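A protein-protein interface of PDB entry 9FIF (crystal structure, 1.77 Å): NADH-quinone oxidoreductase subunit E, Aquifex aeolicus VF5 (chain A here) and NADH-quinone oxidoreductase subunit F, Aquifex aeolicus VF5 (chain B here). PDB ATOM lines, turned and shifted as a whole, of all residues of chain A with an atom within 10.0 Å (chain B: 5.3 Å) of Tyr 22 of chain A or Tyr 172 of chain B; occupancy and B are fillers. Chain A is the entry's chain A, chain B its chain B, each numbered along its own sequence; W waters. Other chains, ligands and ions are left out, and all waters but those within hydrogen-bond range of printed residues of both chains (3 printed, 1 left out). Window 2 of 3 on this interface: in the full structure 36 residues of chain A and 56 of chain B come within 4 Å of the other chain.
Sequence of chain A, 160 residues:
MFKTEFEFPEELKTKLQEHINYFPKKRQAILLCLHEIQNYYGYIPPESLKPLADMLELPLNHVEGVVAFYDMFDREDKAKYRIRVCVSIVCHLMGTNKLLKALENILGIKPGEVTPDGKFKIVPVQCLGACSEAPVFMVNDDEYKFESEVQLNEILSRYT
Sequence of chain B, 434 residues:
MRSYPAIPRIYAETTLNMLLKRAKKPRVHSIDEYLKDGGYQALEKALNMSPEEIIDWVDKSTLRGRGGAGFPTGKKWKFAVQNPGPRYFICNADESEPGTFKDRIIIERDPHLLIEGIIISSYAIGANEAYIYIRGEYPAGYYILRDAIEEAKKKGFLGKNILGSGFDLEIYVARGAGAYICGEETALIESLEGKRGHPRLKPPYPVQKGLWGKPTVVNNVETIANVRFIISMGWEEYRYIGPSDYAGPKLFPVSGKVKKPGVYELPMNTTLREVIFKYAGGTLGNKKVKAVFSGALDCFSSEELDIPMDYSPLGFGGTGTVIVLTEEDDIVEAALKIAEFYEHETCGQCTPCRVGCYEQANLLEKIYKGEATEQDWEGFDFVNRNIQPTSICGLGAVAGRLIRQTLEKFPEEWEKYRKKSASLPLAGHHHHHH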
ATOM      1  N   THR A  14      30.308  25.993  -6.676  1.00  0.00           N
ATOM      2  CA  THR A  14      31.335  25.132  -6.110  1.00  0.00           C
ATOM      3  C   THR A  14      31.136  25.026  -4.599  1.00  0.00           C
ATOM      4  O   THR A  14      31.145  23.929  -4.047  1.00  0.00           O
ATOM      5  CB  THR A  14      32.716  25.668  -6.486  1.00  0.00           C
ATOM      6  OG1 THR A  14      32.806  25.365  -7.872  1.00  0.00           O
ATOM      7  CG2 THR A  14      33.854  24.980  -5.753  1.00  0.00           C
ATOM      8  N   LYS A  15      30.903  26.160  -3.931  1.00  0.00           N
ATOM      9  CA  LYS A  15      30.785  26.155  -2.484  1.00  0.00           C
ATOM     10  C   LYS A  15      29.508  25.426  -2.042  1.00  0.00           C
ATOM     11  O   LYS A  15      29.537  24.667  -1.073  1.00  0.00           O
ATOM     12  CB  LYS A  15      30.947  27.584  -1.954  1.00  0.00           C
ATOM     13  CG  LYS A  15      31.289  27.649  -0.478  1.00  0.00           C
ATOM     14  CD  LYS A  15      32.634  27.057  -0.061  1.00  0.00           C
ATOM     15  CE  LYS A  15      32.662  26.657   1.399  1.00  0.00           C
ATOM     16  NZ  LYS A  15      32.312  27.747   2.318  1.00  0.00           N
ATOM     17  N   LEU A  16      28.395  25.634  -2.762  1.00  0.00           N
ATOM     18  CA  LEU A  16      27.152  24.920  -2.486  1.00  0.00           C
ATOM     19  C   LEU A  16      27.360  23.410  -2.622  1.00  0.00           C
ATOM     20  O   LEU A  16      26.849  22.639  -1.812  1.00  0.00           O
ATOM     21  CB  LEU A  16      26.023  25.398  -3.399  1.00  0.00           C
ATOM     22  CG  LEU A  16      25.598  26.859  -3.229  1.00  0.00           C
ATOM     23  CD1 LEU A  16      24.622  27.233  -4.327  1.00  0.00           C
ATOM     24  CD2 LEU A  16      24.997  27.109  -1.861  1.00  0.00           C
ATOM     25  N   GLN A  17      28.140  22.999  -3.624  1.00  0.00           N
ATOM     26  CA  GLN A  17      28.411  21.587  -3.865  1.00  0.00           C
ATOM     27  C   GLN A  17      29.214  20.978  -2.707  1.00  0.00           C
ATOM     28  O   GLN A  17      28.967  19.831  -2.343  1.00  0.00           O
ATOM     29  CB  GLN A  17      29.107  21.406  -5.215  1.00  0.00           C
ATOM     30  CG  GLN A  17      29.076  19.972  -5.732  1.00  0.00           C
ATOM     31  CD  GLN A  17      27.669  19.436  -5.898  1.00  0.00           C
ATOM     32  OE1 GLN A  17      26.880  19.937  -6.708  1.00  0.00           O
ATOM     33  NE2 GLN A  17      27.330  18.422  -5.111  1.00  0.00           N
ATOM     34  N   GLU A  18      30.168  21.737  -2.142  1.00  0.00           N
ATOM     35  CA  GLU A  18      30.931  21.307  -0.973  1.00  0.00           C
ATOM     36  C   GLU A  18      29.970  20.979   0.172  1.00  0.00           C
ATOM     37  O   GLU A  18      30.073  19.923   0.789  1.00  0.00           O
ATOM     38  CB  GLU A  18      31.940  22.351  -0.471  1.00  0.00           C
ATOM     39  CG  GLU A  18      33.217  22.456  -1.306  1.00  0.00           C
ATOM     40  CD  GLU A  18      34.066  23.705  -1.064  1.00  0.00           C
ATOM     41  OE1 GLU A  18      34.689  24.199  -2.036  1.00  0.00           O
ATOM     42  OE2 GLU A  18      34.083  24.210   0.085  1.00  0.00           O
ATOM     43  N   HIS A  19      29.038  21.892   0.448  1.00  0.00           N
ATOM     44  CA  HIS A  19      28.070  21.691   1.513  1.00  0.00           C
ATOM     45  C   HIS A  19      27.246  20.436   1.244  1.00  0.00           C
ATOM     46  O   HIS A  19      27.068  19.605   2.126  1.00  0.00           O
ATOM     47  CB  HIS A  19      27.156  22.914   1.642  1.00  0.00           C
ATOM     48  CG  HIS A  19      27.846  24.138   2.129  1.00  0.00           C
ATOM     49  ND1 HIS A  19      28.691  24.140   3.214  1.00  0.00           N
ATOM     50  CD2 HIS A  19      27.768  25.404   1.707  1.00  0.00           C
ATOM     51  CE1 HIS A  19      29.113  25.381   3.430  1.00  0.00           C
ATOM     52  NE2 HIS A  19      28.573  26.167   2.513  1.00  0.00           N
ATOM     53  N   ILE A  20      26.734  20.317   0.021  1.00  0.00           N
ATOM     54  CA  ILE A  20      25.866  19.210  -0.349  1.00  0.00           C
ATOM     55  C   ILE A  20      26.608  17.876  -0.235  1.00  0.00           C
ATOM     56  O   ILE A  20      25.980  16.865   0.066  1.00  0.00           O
ATOM     57  CB  ILE A  20      25.270  19.465  -1.748  1.00  0.00           C
ATOM     58  CG1 ILE A  20      24.170  20.519  -1.655  1.00  0.00           C
ATOM     59  CG2 ILE A  20      24.780  18.181  -2.418  1.00  0.00           C
ATOM     60  CD1 ILE A  20      23.715  21.065  -2.995  1.00  0.00           C
ATOM     61  N   ASN A  21      27.928  17.878  -0.463  1.00  0.00           N
ATOM     62  CA  ASN A  21      28.740  16.671  -0.385  1.00  0.00           C
ATOM     63  C   ASN A  21      29.187  16.366   1.050  1.00  0.00           C
ATOM     64  O   ASN A  21      29.716  15.287   1.314  1.00  0.00           O
ATOM     65  CB  ASN A  21      29.944  16.784  -1.315  1.00  0.00           C
ATOM     66  CG  ASN A  21      29.544  16.700  -2.769  1.00  0.00           C
ATOM     67  OD1 ASN A  21      28.467  16.191  -3.081  1.00  0.00           O
ATOM     68  ND2 ASN A  21      30.396  17.144  -3.680  1.00  0.00           N
ATOM     69  N   TYR A  22      28.979  17.309   1.974  1.00  0.00           N
ATOM     70  CA  TYR A  22      29.551  17.228   3.315  1.00  0.00           C
ATOM     71  C   TYR A  22      28.803  16.227   4.195  1.00  0.00           C
ATOM     72  O   TYR A  22      29.440  15.426   4.867  1.00  0.00           O
ATOM     73  CB  TYR A  22      29.514  18.611   3.970  1.00  0.00           C
ATOM     74  CG  TYR A  22      29.947  18.693   5.431  1.00  0.00           C
ATOM     75  CD1 TYR A  22      31.286  18.577   5.800  1.00  0.00           C
ATOM     76  CD2 TYR A  22      29.025  18.965   6.429  1.00  0.00           C
ATOM     77  CE1 TYR A  22      31.686  18.698   7.123  1.00  0.00           C
ATOM     78  CE2 TYR A  22      29.410  19.073   7.754  1.00  0.00           C
ATOM     79  CZ  TYR A  22      30.742  18.937   8.104  1.00  0.00           C
ATOM     80  OH  TYR A  22      31.127  19.084   9.396  1.00  0.00           O
ATOM     81  N   PHE A  23      27.470  16.333   4.263  1.00  0.00           N
ATOM     82  CA  PHE A  23      26.676  15.438   5.093  1.00  0.00           C
ATOM     83  C   PHE A  23      26.411  14.133   4.340  1.00  0.00           C
ATOM     84  O   PHE A  23      26.550  14.066   3.115  1.00  0.00           O
ATOM     85  CB  PHE A  23      25.338  16.038   5.530  1.00  0.00           C
ATOM     86  CG  PHE A  23      25.435  17.318   6.343  1.00  0.00           C
ATOM     87  CD1 PHE A  23      25.702  17.276   7.707  1.00  0.00           C
ATOM     88  CD2 PHE A  23      25.256  18.555   5.746  1.00  0.00           C
ATOM     89  CE1 PHE A  23      25.793  18.439   8.450  1.00  0.00           C
ATOM     90  CE2 PHE A  23      25.347  19.716   6.502  1.00  0.00           C
ATOM     91  CZ  PHE A  23      25.601  19.655   7.850  1.00  0.00           C
ATOM     92  N   PRO A  24      26.038  13.035   5.045  1.00  0.00           N
ATOM     93  CA  PRO A  24      25.673  11.790   4.366  1.00  0.00           C
ATOM     94  C   PRO A  24      24.560  11.931   3.332  1.00  0.00           C
ATOM     95  O   PRO A  24      24.629  11.291   2.304  1.00  0.00           O
ATOM     96  CB  PRO A  24      25.268  10.861   5.514  1.00  0.00           C
ATOM     97  CG  PRO A  24      26.059  11.388   6.686  1.00  0.00           C
ATOM     98  CD  PRO A  24      26.056  12.897   6.509  1.00  0.00           C
ATOM     99  N   LYS A  25      23.538  12.763   3.602  1.00  0.00           N
ATOM    100  CA  LYS A  25      22.457  12.964   2.645  1.00  0.00           C
ATOM    101  C   LYS A  25      22.449  14.418   2.181  1.00  0.00           C
ATOM    102  O   LYS A  25      22.697  15.328   2.970  1.00  0.00           O
ATOM    103  CB  LYS A  25      21.101  12.573   3.245  1.00  0.00           C
ATOM    104  CG  LYS A  25      21.070  11.219   3.934  1.00  0.00           C
ATOM    105  CD  LYS A  25      19.670  10.688   4.215  1.00  0.00           C
ATOM    106  CE  LYS A  25      19.697   9.325   4.846  1.00  0.00           C
ATOM    107  NZ  LYS A  25      18.352   8.778   5.052  1.00  0.00           N
ATOM    108  N   LYS A  26      22.130  14.629   0.897  1.00  0.00           N
ATOM    109  CA  LYS A  26      22.221  15.949   0.296  1.00  0.00           C
ATOM    110  C   LYS A  26      21.320  16.947   1.023  1.00  0.00           C
ATOM    111  O   LYS A  26      21.709  18.094   1.242  1.00  0.00           O
ATOM    112  CB  LYS A  26      21.816  15.931  -1.184  1.00  0.00           C
ATOM    113  CG  LYS A  26      22.737  15.150  -2.114  1.00  0.00           C
ATOM    114  CD  LYS A  26      22.317  15.232  -3.578  1.00  0.00           C
ATOM    115  CE  LYS A  26      23.340  14.715  -4.549  1.00  0.00           C
ATOM    116  NZ  LYS A  26      23.728  13.335  -4.244  1.00  0.00           N
ATOM    117  N   ARG A  27      20.110  16.506   1.394  1.00  0.00           N
ATOM    118  CA  ARG A  27      19.093  17.426   1.878  1.00  0.00           C
ATOM    119  C   ARG A  27      19.474  18.000   3.233  1.00  0.00           C
ATOM    120  O   ARG A  27      18.911  19.005   3.657  1.00  0.00           O
ATOM    121  CB  ARG A  27      17.695  16.808   1.966  1.00  0.00           C
ATOM    122  CG  ARG A  27      17.525  15.626   2.910  1.00  0.00           C
ATOM    123  CD  ARG A  27      16.278  14.878   2.486  1.00  0.00           C
ATOM    124  NE  ARG A  27      16.026  13.643   3.230  1.00  0.00           N
ATOM    125  CZ  ARG A  27      16.364  12.431   2.805  1.00  0.00           C
ATOM    126  NH1 ARG A  27      15.831  11.359   3.364  1.00  0.00           N
ATOM    127  NH2 ARG A  27      17.193  12.295   1.789  1.00  0.00           N
ATOM    128  N   GLN A  28      20.431  17.365   3.917  1.00  0.00           N
ATOM    129  CA  GLN A  28      20.869  17.855   5.208  1.00  0.00           C
ATOM    130  C   GLN A  28      21.598  19.190   5.070  1.00  0.00           C
ATOM    131  O   GLN A  28      21.687  19.910   6.052  1.00  0.00           O
ATOM    132  CB  GLN A  28      21.769  16.851   5.923  1.00  0.00           C
ATOM    133  CG  GLN A  28      21.109  15.494   6.109  1.00  0.00           C
ATOM    134  CD  GLN A  28      21.930  14.573   6.973  1.00  0.00           C
ATOM    135  OE1 GLN A  28      22.614  13.665   6.481  1.00  0.00           O
ATOM    136  NE2 GLN A  28      21.868  14.814   8.270  1.00  0.00           N
ATOM    137  N   ALA A  29      22.073  19.522   3.859  1.00  0.00           N
ATOM    138  CA  ALA A  29      22.869  20.717   3.612  1.00  0.00           C
ATOM    139  C   ALA A  29      22.048  21.985   3.374  1.00  0.00           C
ATOM    140  O   ALA A  29      22.631  23.019   3.058  1.00  0.00           O
ATOM    141  CB  ALA A  29      23.751  20.474   2.413  1.00  0.00           C
ATOM    142  N   ILE A  30      20.717  21.922   3.497  1.00  0.00           N
ATOM    143  CA  ILE A  30      19.858  23.012   3.057  1.00  0.00           C
ATOM    144  C   ILE A  30      20.176  24.327   3.784  1.00  0.00           C
ATOM    145  O   ILE A  30      20.241  25.373   3.133  1.00  0.00           O
ATOM    146  CB  ILE A  30      18.359  22.651   3.145  1.00  0.00           C
ATOM    147  CG1 ILE A  30      17.494  23.793   2.588  1.00  0.00           C
ATOM    148  CG2 ILE A  30      17.919  22.256   4.561  1.00  0.00           C
ATOM    149  CD1 ILE A  30      16.055  23.399   2.308  1.00  0.00           C
ATOM    150  N   LEU A  32      23.039  25.232   5.445  1.00  0.00           N
ATOM    151  CA  LEU A  32      24.369  25.702   5.088  1.00  0.00           C
ATOM    152  C   LEU A  32      24.337  26.369   3.719  1.00  0.00           C
ATOM    153  O   LEU A  32      24.996  27.385   3.516  1.00  0.00           O
ATOM    154  CB  LEU A  32      25.400  24.577   5.109  1.00  0.00           C
ATOM    155  CG  LEU A  32      25.841  24.103   6.494  1.00  0.00           C
ATOM    156  CD1 LEU A  32      26.762  22.921   6.311  1.00  0.00           C
ATOM    157  CD2 LEU A  32      26.550  25.220   7.231  1.00  0.00           C
ATOM    158  N   CYS A  33      23.596  25.773   2.781  1.00  0.00           N
ATOM    159  CA  CYS A  33      23.454  26.329   1.445  1.00  0.00           C
ATOM    160  C   CYS A  33      22.795  27.709   1.485  1.00  0.00           C
ATOM    161  O   CYS A  33      23.257  28.635   0.824  1.00  0.00           O
ATOM    162  CB  CYS A  33      22.662  25.385   0.555  1.00  0.00           C
ATOM    163  SG  CYS A  33      23.650  23.985  -0.020  1.00  0.00           S
ATOM    164  N   LEU A  56      19.619  19.933  -4.223  1.00  0.00           N
ATOM    165  CA  LEU A  56      19.325  19.238  -2.978  1.00  0.00           C
ATOM    166  C   LEU A  56      18.426  18.031  -3.231  1.00  0.00           C
ATOM    167  O   LEU A  56      18.190  17.262  -2.304  1.00  0.00           O
ATOM    168  CB  LEU A  56      18.649  20.201  -2.005  1.00  0.00           C
ATOM    169  CG  LEU A  56      19.495  21.369  -1.498  1.00  0.00           C
ATOM    170  CD1 LEU A  56      18.616  22.353  -0.746  1.00  0.00           C
ATOM    171  CD2 LEU A  56      20.610  20.855  -0.618  1.00  0.00           C
ATOM    172  N   GLU B 129      28.414   8.012  13.602  1.00  0.00           N
ATOM    173  CA  GLU B 129      28.077   9.283  12.997  1.00  0.00           C
ATOM    174  C   GLU B 129      27.536  10.164  14.114  1.00  0.00           C
ATOM    175  O   GLU B 129      26.576   9.785  14.779  1.00  0.00           O
ATOM    176  CB  GLU B 129      27.053   9.001  11.897  1.00  0.00           C
ATOM    177  CG  GLU B 129      26.459  10.242  11.235  1.00  0.00           C
ATOM    178  CD  GLU B 129      25.528   9.944  10.064  1.00  0.00           C
ATOM    179  OE1 GLU B 129      25.799   8.961   9.350  1.00  0.00           O
ATOM    180  OE2 GLU B 129      24.561  10.718   9.840  1.00  0.00           O
ATOM    181  N   ALA B 130      28.178  11.307  14.333  1.00  0.00           N
ATOM    182  CA  ALA B 130      27.732  12.260  15.328  1.00  0.00           C
ATOM    183  C   ALA B 130      27.601  13.639  14.701  1.00  0.00           C
ATOM    184  O   ALA B 130      28.227  13.940  13.684  1.00  0.00           O
ATOM    185  CB  ALA B 130      28.688  12.307  16.497  1.00  0.00           C
ATOM    186  N   TYR B 131      26.805  14.479  15.359  1.00  0.00           N
ATOM    187  CA  TYR B 131      26.545  15.820  14.875  1.00  0.00           C
ATOM    188  C   TYR B 131      26.735  16.801  16.016  1.00  0.00           C
ATOM    189  O   TYR B 131      26.494  16.447  17.168  1.00  0.00           O
ATOM    190  CB  TYR B 131      25.097  15.955  14.411  1.00  0.00           C
ATOM    191  CG  TYR B 131      24.816  15.124  13.177  1.00  0.00           C
ATOM    192  CD1 TYR B 131      24.540  13.767  13.254  1.00  0.00           C
ATOM    193  CD2 TYR B 131      24.866  15.720  11.925  1.00  0.00           C
ATOM    194  CE1 TYR B 131      24.308  13.025  12.108  1.00  0.00           C
ATOM    195  CE2 TYR B 131      24.641  14.992  10.779  1.00  0.00           C
ATOM    196  CZ  TYR B 131      24.357  13.646  10.872  1.00  0.00           C
ATOM    197  OH  TYR B 131      24.129  12.995   9.708  1.00  0.00           O
ATOM    198  N   ILE B 132      27.196  18.002  15.667  1.00  0.00           N
ATOM    199  CA  ILE B 132      26.988  19.184  16.487  1.00  0.00           C
ATOM    200  C   ILE B 132      25.996  20.074  15.742  1.00  0.00           C
ATOM    201  O   ILE B 132      26.234  20.421  14.590  1.00  0.00           O
ATOM    202  CB  ILE B 132      28.306  19.931  16.748  1.00  0.00           C
ATOM    203  CG1 ILE B 132      29.335  19.054  17.455  1.00  0.00           C
ATOM    204  CG2 ILE B 132      28.037  21.227  17.525  1.00  0.00           C
ATOM    205  CD1 ILE B 132      30.732  19.639  17.454  1.00  0.00           C
ATOM    206  N   ARG B 146      34.787  23.515  13.363  1.00  0.00           N
ATOM    207  CA  ARG B 146      35.190  22.865  12.126  1.00  0.00           C
ATOM    208  C   ARG B 146      36.708  22.682  12.134  1.00  0.00           C
ATOM    209  O   ARG B 146      37.217  21.624  11.766  1.00  0.00           O
ATOM    210  CB  ARG B 146      34.786  23.667  10.881  1.00  0.00           C
ATOM    211  CG  ARG B 146      33.311  23.589  10.520  1.00  0.00           C
ATOM    212  CD  ARG B 146      32.878  22.206  10.039  1.00  0.00           C
ATOM    213  NE  ARG B 146      33.709  21.734   8.926  1.00  0.00           N
ATOM    214  CZ  ARG B 146      33.383  21.755   7.635  1.00  0.00           C
ATOM    215  NH1 ARG B 146      32.253  22.293   7.232  1.00  0.00           N
ATOM    216  NH2 ARG B 146      34.206  21.247   6.739  1.00  0.00           N
ATOM    217  N   GLU B 170      32.774   9.968  12.468  1.00  0.00           N
ATOM    218  CA  GLU B 170      32.817  11.290  11.852  1.00  0.00           C
ATOM    219  C   GLU B 170      31.874  12.184  12.645  1.00  0.00           C
ATOM    220  O   GLU B 170      30.812  11.723  13.058  1.00  0.00           O
ATOM    221  CB  GLU B 170      32.393  11.304  10.379  1.00  0.00           C
ATOM    222  CG  GLU B 170      33.257  10.444   9.453  1.00  0.00           C
ATOM    223  CD  GLU B 170      34.717  10.862   9.326  1.00  0.00           C
ATOM    224  OE1 GLU B 170      35.060  12.027   9.668  1.00  0.00           O
ATOM    225  OE2 GLU B 170      35.540   9.993   8.930  1.00  0.00           O
ATOM    226  N   ILE B 171      32.283  13.445  12.857  1.00  0.00           N
ATOM    227  CA  ILE B 171      31.476  14.467  13.499  1.00  0.00           C
ATOM    228  C   ILE B 171      31.168  15.545  12.457  1.00  0.00           C
ATOM    229  O   ILE B 171      32.082  16.174  11.931  1.00  0.00           O
ATOM    230  CB  ILE B 171      32.153  15.069  14.742  1.00  0.00           C
ATOM    231  CG1 ILE B 171      32.506  14.000  15.789  1.00  0.00           C
ATOM    232  CG2 ILE B 171      31.262  16.156  15.345  1.00  0.00           C
ATOM    233  CD1 ILE B 171      33.322  14.527  16.961  1.00  0.00           C
ATOM    234  N   TYR B 172      29.877  15.719  12.155  1.00  0.00           N
ATOM    235  CA  TYR B 172      29.405  16.720  11.212  1.00  0.00           C
ATOM    236  C   TYR B 172      28.913  17.926  12.004  1.00  0.00           C
ATOM    237  O   TYR B 172      28.286  17.755  13.046  1.00  0.00           O
ATOM    238  CB  TYR B 172      28.274  16.142  10.364  1.00  0.00           C
ATOM    239  CG  TYR B 172      28.705  14.897   9.611  1.00  0.00           C
ATOM    240  CD1 TYR B 172      29.362  15.010   8.394  1.00  0.00           C
ATOM    241  CD2 TYR B 172      28.484  13.623  10.123  1.00  0.00           C
ATOM    242  CE1 TYR B 172      29.787  13.891   7.693  1.00  0.00           C
ATOM    243  CE2 TYR B 172      28.906  12.495   9.432  1.00  0.00           C
ATOM    244  CZ  TYR B 172      29.552  12.632   8.212  1.00  0.00           C
ATOM    245  OH  TYR B 172      29.993  11.564   7.485  1.00  0.00           O
ATOM    246  N   VAL B 173      29.198  19.128  11.498  1.00  0.00           N
ATOM    247  CA  VAL B 173      28.734  20.351  12.142  1.00  0.00           C
ATOM    248  C   VAL B 173      27.624  20.958  11.285  1.00  0.00           C
ATOM    249  O   VAL B 173      27.836  21.338  10.121  1.00  0.00           O
ATOM    250  CB  VAL B 173      29.838  21.392  12.411  1.00  0.00           C
ATOM    251  CG1 VAL B 173      29.311  22.537  13.275  1.00  0.00           C
ATOM    252  CG2 VAL B 173      31.088  20.766  13.030  1.00  0.00           C
ATOM    253  N   ALA B 174      26.432  21.039  11.889  1.00  0.00           N
ATOM    254  CA  ALA B 174      25.278  21.659  11.258  1.00  0.00           C
ATOM    255  C   ALA B 174      25.008  23.005  11.924  1.00  0.00           C
ATOM    256  O   ALA B 174      25.318  23.191  13.102  1.00  0.00           O
ATOM    257  CB  ALA B 174      24.073  20.754  11.376  1.00  0.00           C
HETATM  258  O   HOH W   1      29.157  12.088   4.578  1.00  0.00           O
HETATM  259  O   HOH W   2      22.642  11.219   7.810  1.00  0.00           O
HETATM  260  O   HOH W   3      33.435  18.490  10.135  1.00  0.00           O
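Water W3 lies within hydrogen-bond range of OH of Tyr 22 of chain A, O of Ile 171 of chain B and NE of Arg 146 of chain B. Water W2 lies within hydrogen-bond range of OE1 of Gln 28 of chain A (2.8 Å), OE2 of Glu 129 of chain B (2.8 Å) and OH of Tyr 131 of chain B (3.0 Å). Water W1 lies within hydrogen-bond range of OH of Tyr 172 of chain B (3.1 Å) and O of Tyr 22 of chain A (3.4 Å).
N of Val 173 of chain B is in hydrogen-bond range of OH of Tyr 22 of chain A (2.9 Å). The side-chain hydroxyl (OH) of Tyr 131 of chain B sits at hydrogen-bond distance from the side-chain amide nitrogen (NE2) of Gln 28 of chain A, at 3.2 Å.
CE1 of Tyr 22 of chain A touches CZ of Arg 146 of chain B (3.5 Å). Tyr 22 of chain A touches Ile 171 of chain B. CE1 of Tyr 172 of chain B touches O of Tyr 22 of chain A, at 3.2 Å. Phe 23 of chain A touches Tyr 131 of chain B (CD1 to CE2, 3.97 Å). CB of Tyr 172 of chain B touches CD1 of Phe 23 of chain A, at 3.9 Å. Phe 23 of chain A touches Val 173 of chain B. Ala 174 of chain B touches Phe 23 of chain A (CA to CZ, 3.97 Å). Pro 24 of chain A touches Glu 129 of chain B (CG to OE2, 3.6 Å). Pro 24 of chain A touches Tyr 131 of chain B. CZ of Tyr 172 of chain B touches CD of Pro 24 of chain A, 3.9 Å away.
Tyr 22 of chain A touches just these residues of chain B: Arg 146, Ile 171, Tyr 172 and Val 173. Of the printed residues of chain B, Gln 28 of chain A touches Tyr 131 (3.2 Å). Of chain A, only Phe 23 (3.97 Å), Pro 24 (3.7 Å) and Gln 28 (3.2 Å) come within 4 Å of Tyr 131 of chain B. No residue of chain A comes within 4 Å of Glu 170 of chain B. Printed residues of chain A within 4 Å of Ile 171 of chain B: Tyr 22. Of chain A, only Tyr 22, Phe 23 and Pro 24 come within 4 Å of Tyr 172 of chain B. Of chain A, only Tyr 22 (2.9 Å) and Phe 23 (3.6 Å) come within 4 Å of Val 173 of chain B. The nearest residue of chain A that does not touch Tyr 172 of chain B is Asn 21 of chain A (6.5 Å).
OE1 of Gln 28 of chain A is in hydrogen-bond range of N of Lys 25 of chain A (3.2 Å). The backbone NH (N) of Tyr 172 of chain B is in hydrogen-bond range of the backbone carbonyl oxygen (O) of Ala 130 of chain B. The backbone NH (N) of Ile 132 of chain B is in hydrogen-bond range of the backbone carbonyl oxygen (O) of Tyr 172 of chain B (2.8 Å). O of Ile 132 of chain B sits at hydrogen-bond distance from N of Ala 174 of chain B (2.8 Å).
Of the 10 printed residues of chain B, 7 touch a printed residue of chain A. Hydrophobic or aromatic side chains of chain B that line the printed part of chain A: Tyr 131, Tyr 172 and Ala 174. Among the printed residues, no Asp or Glu carboxylate lies within 4 Å of a Lys or Arg side-chain nitrogen of the other chain.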
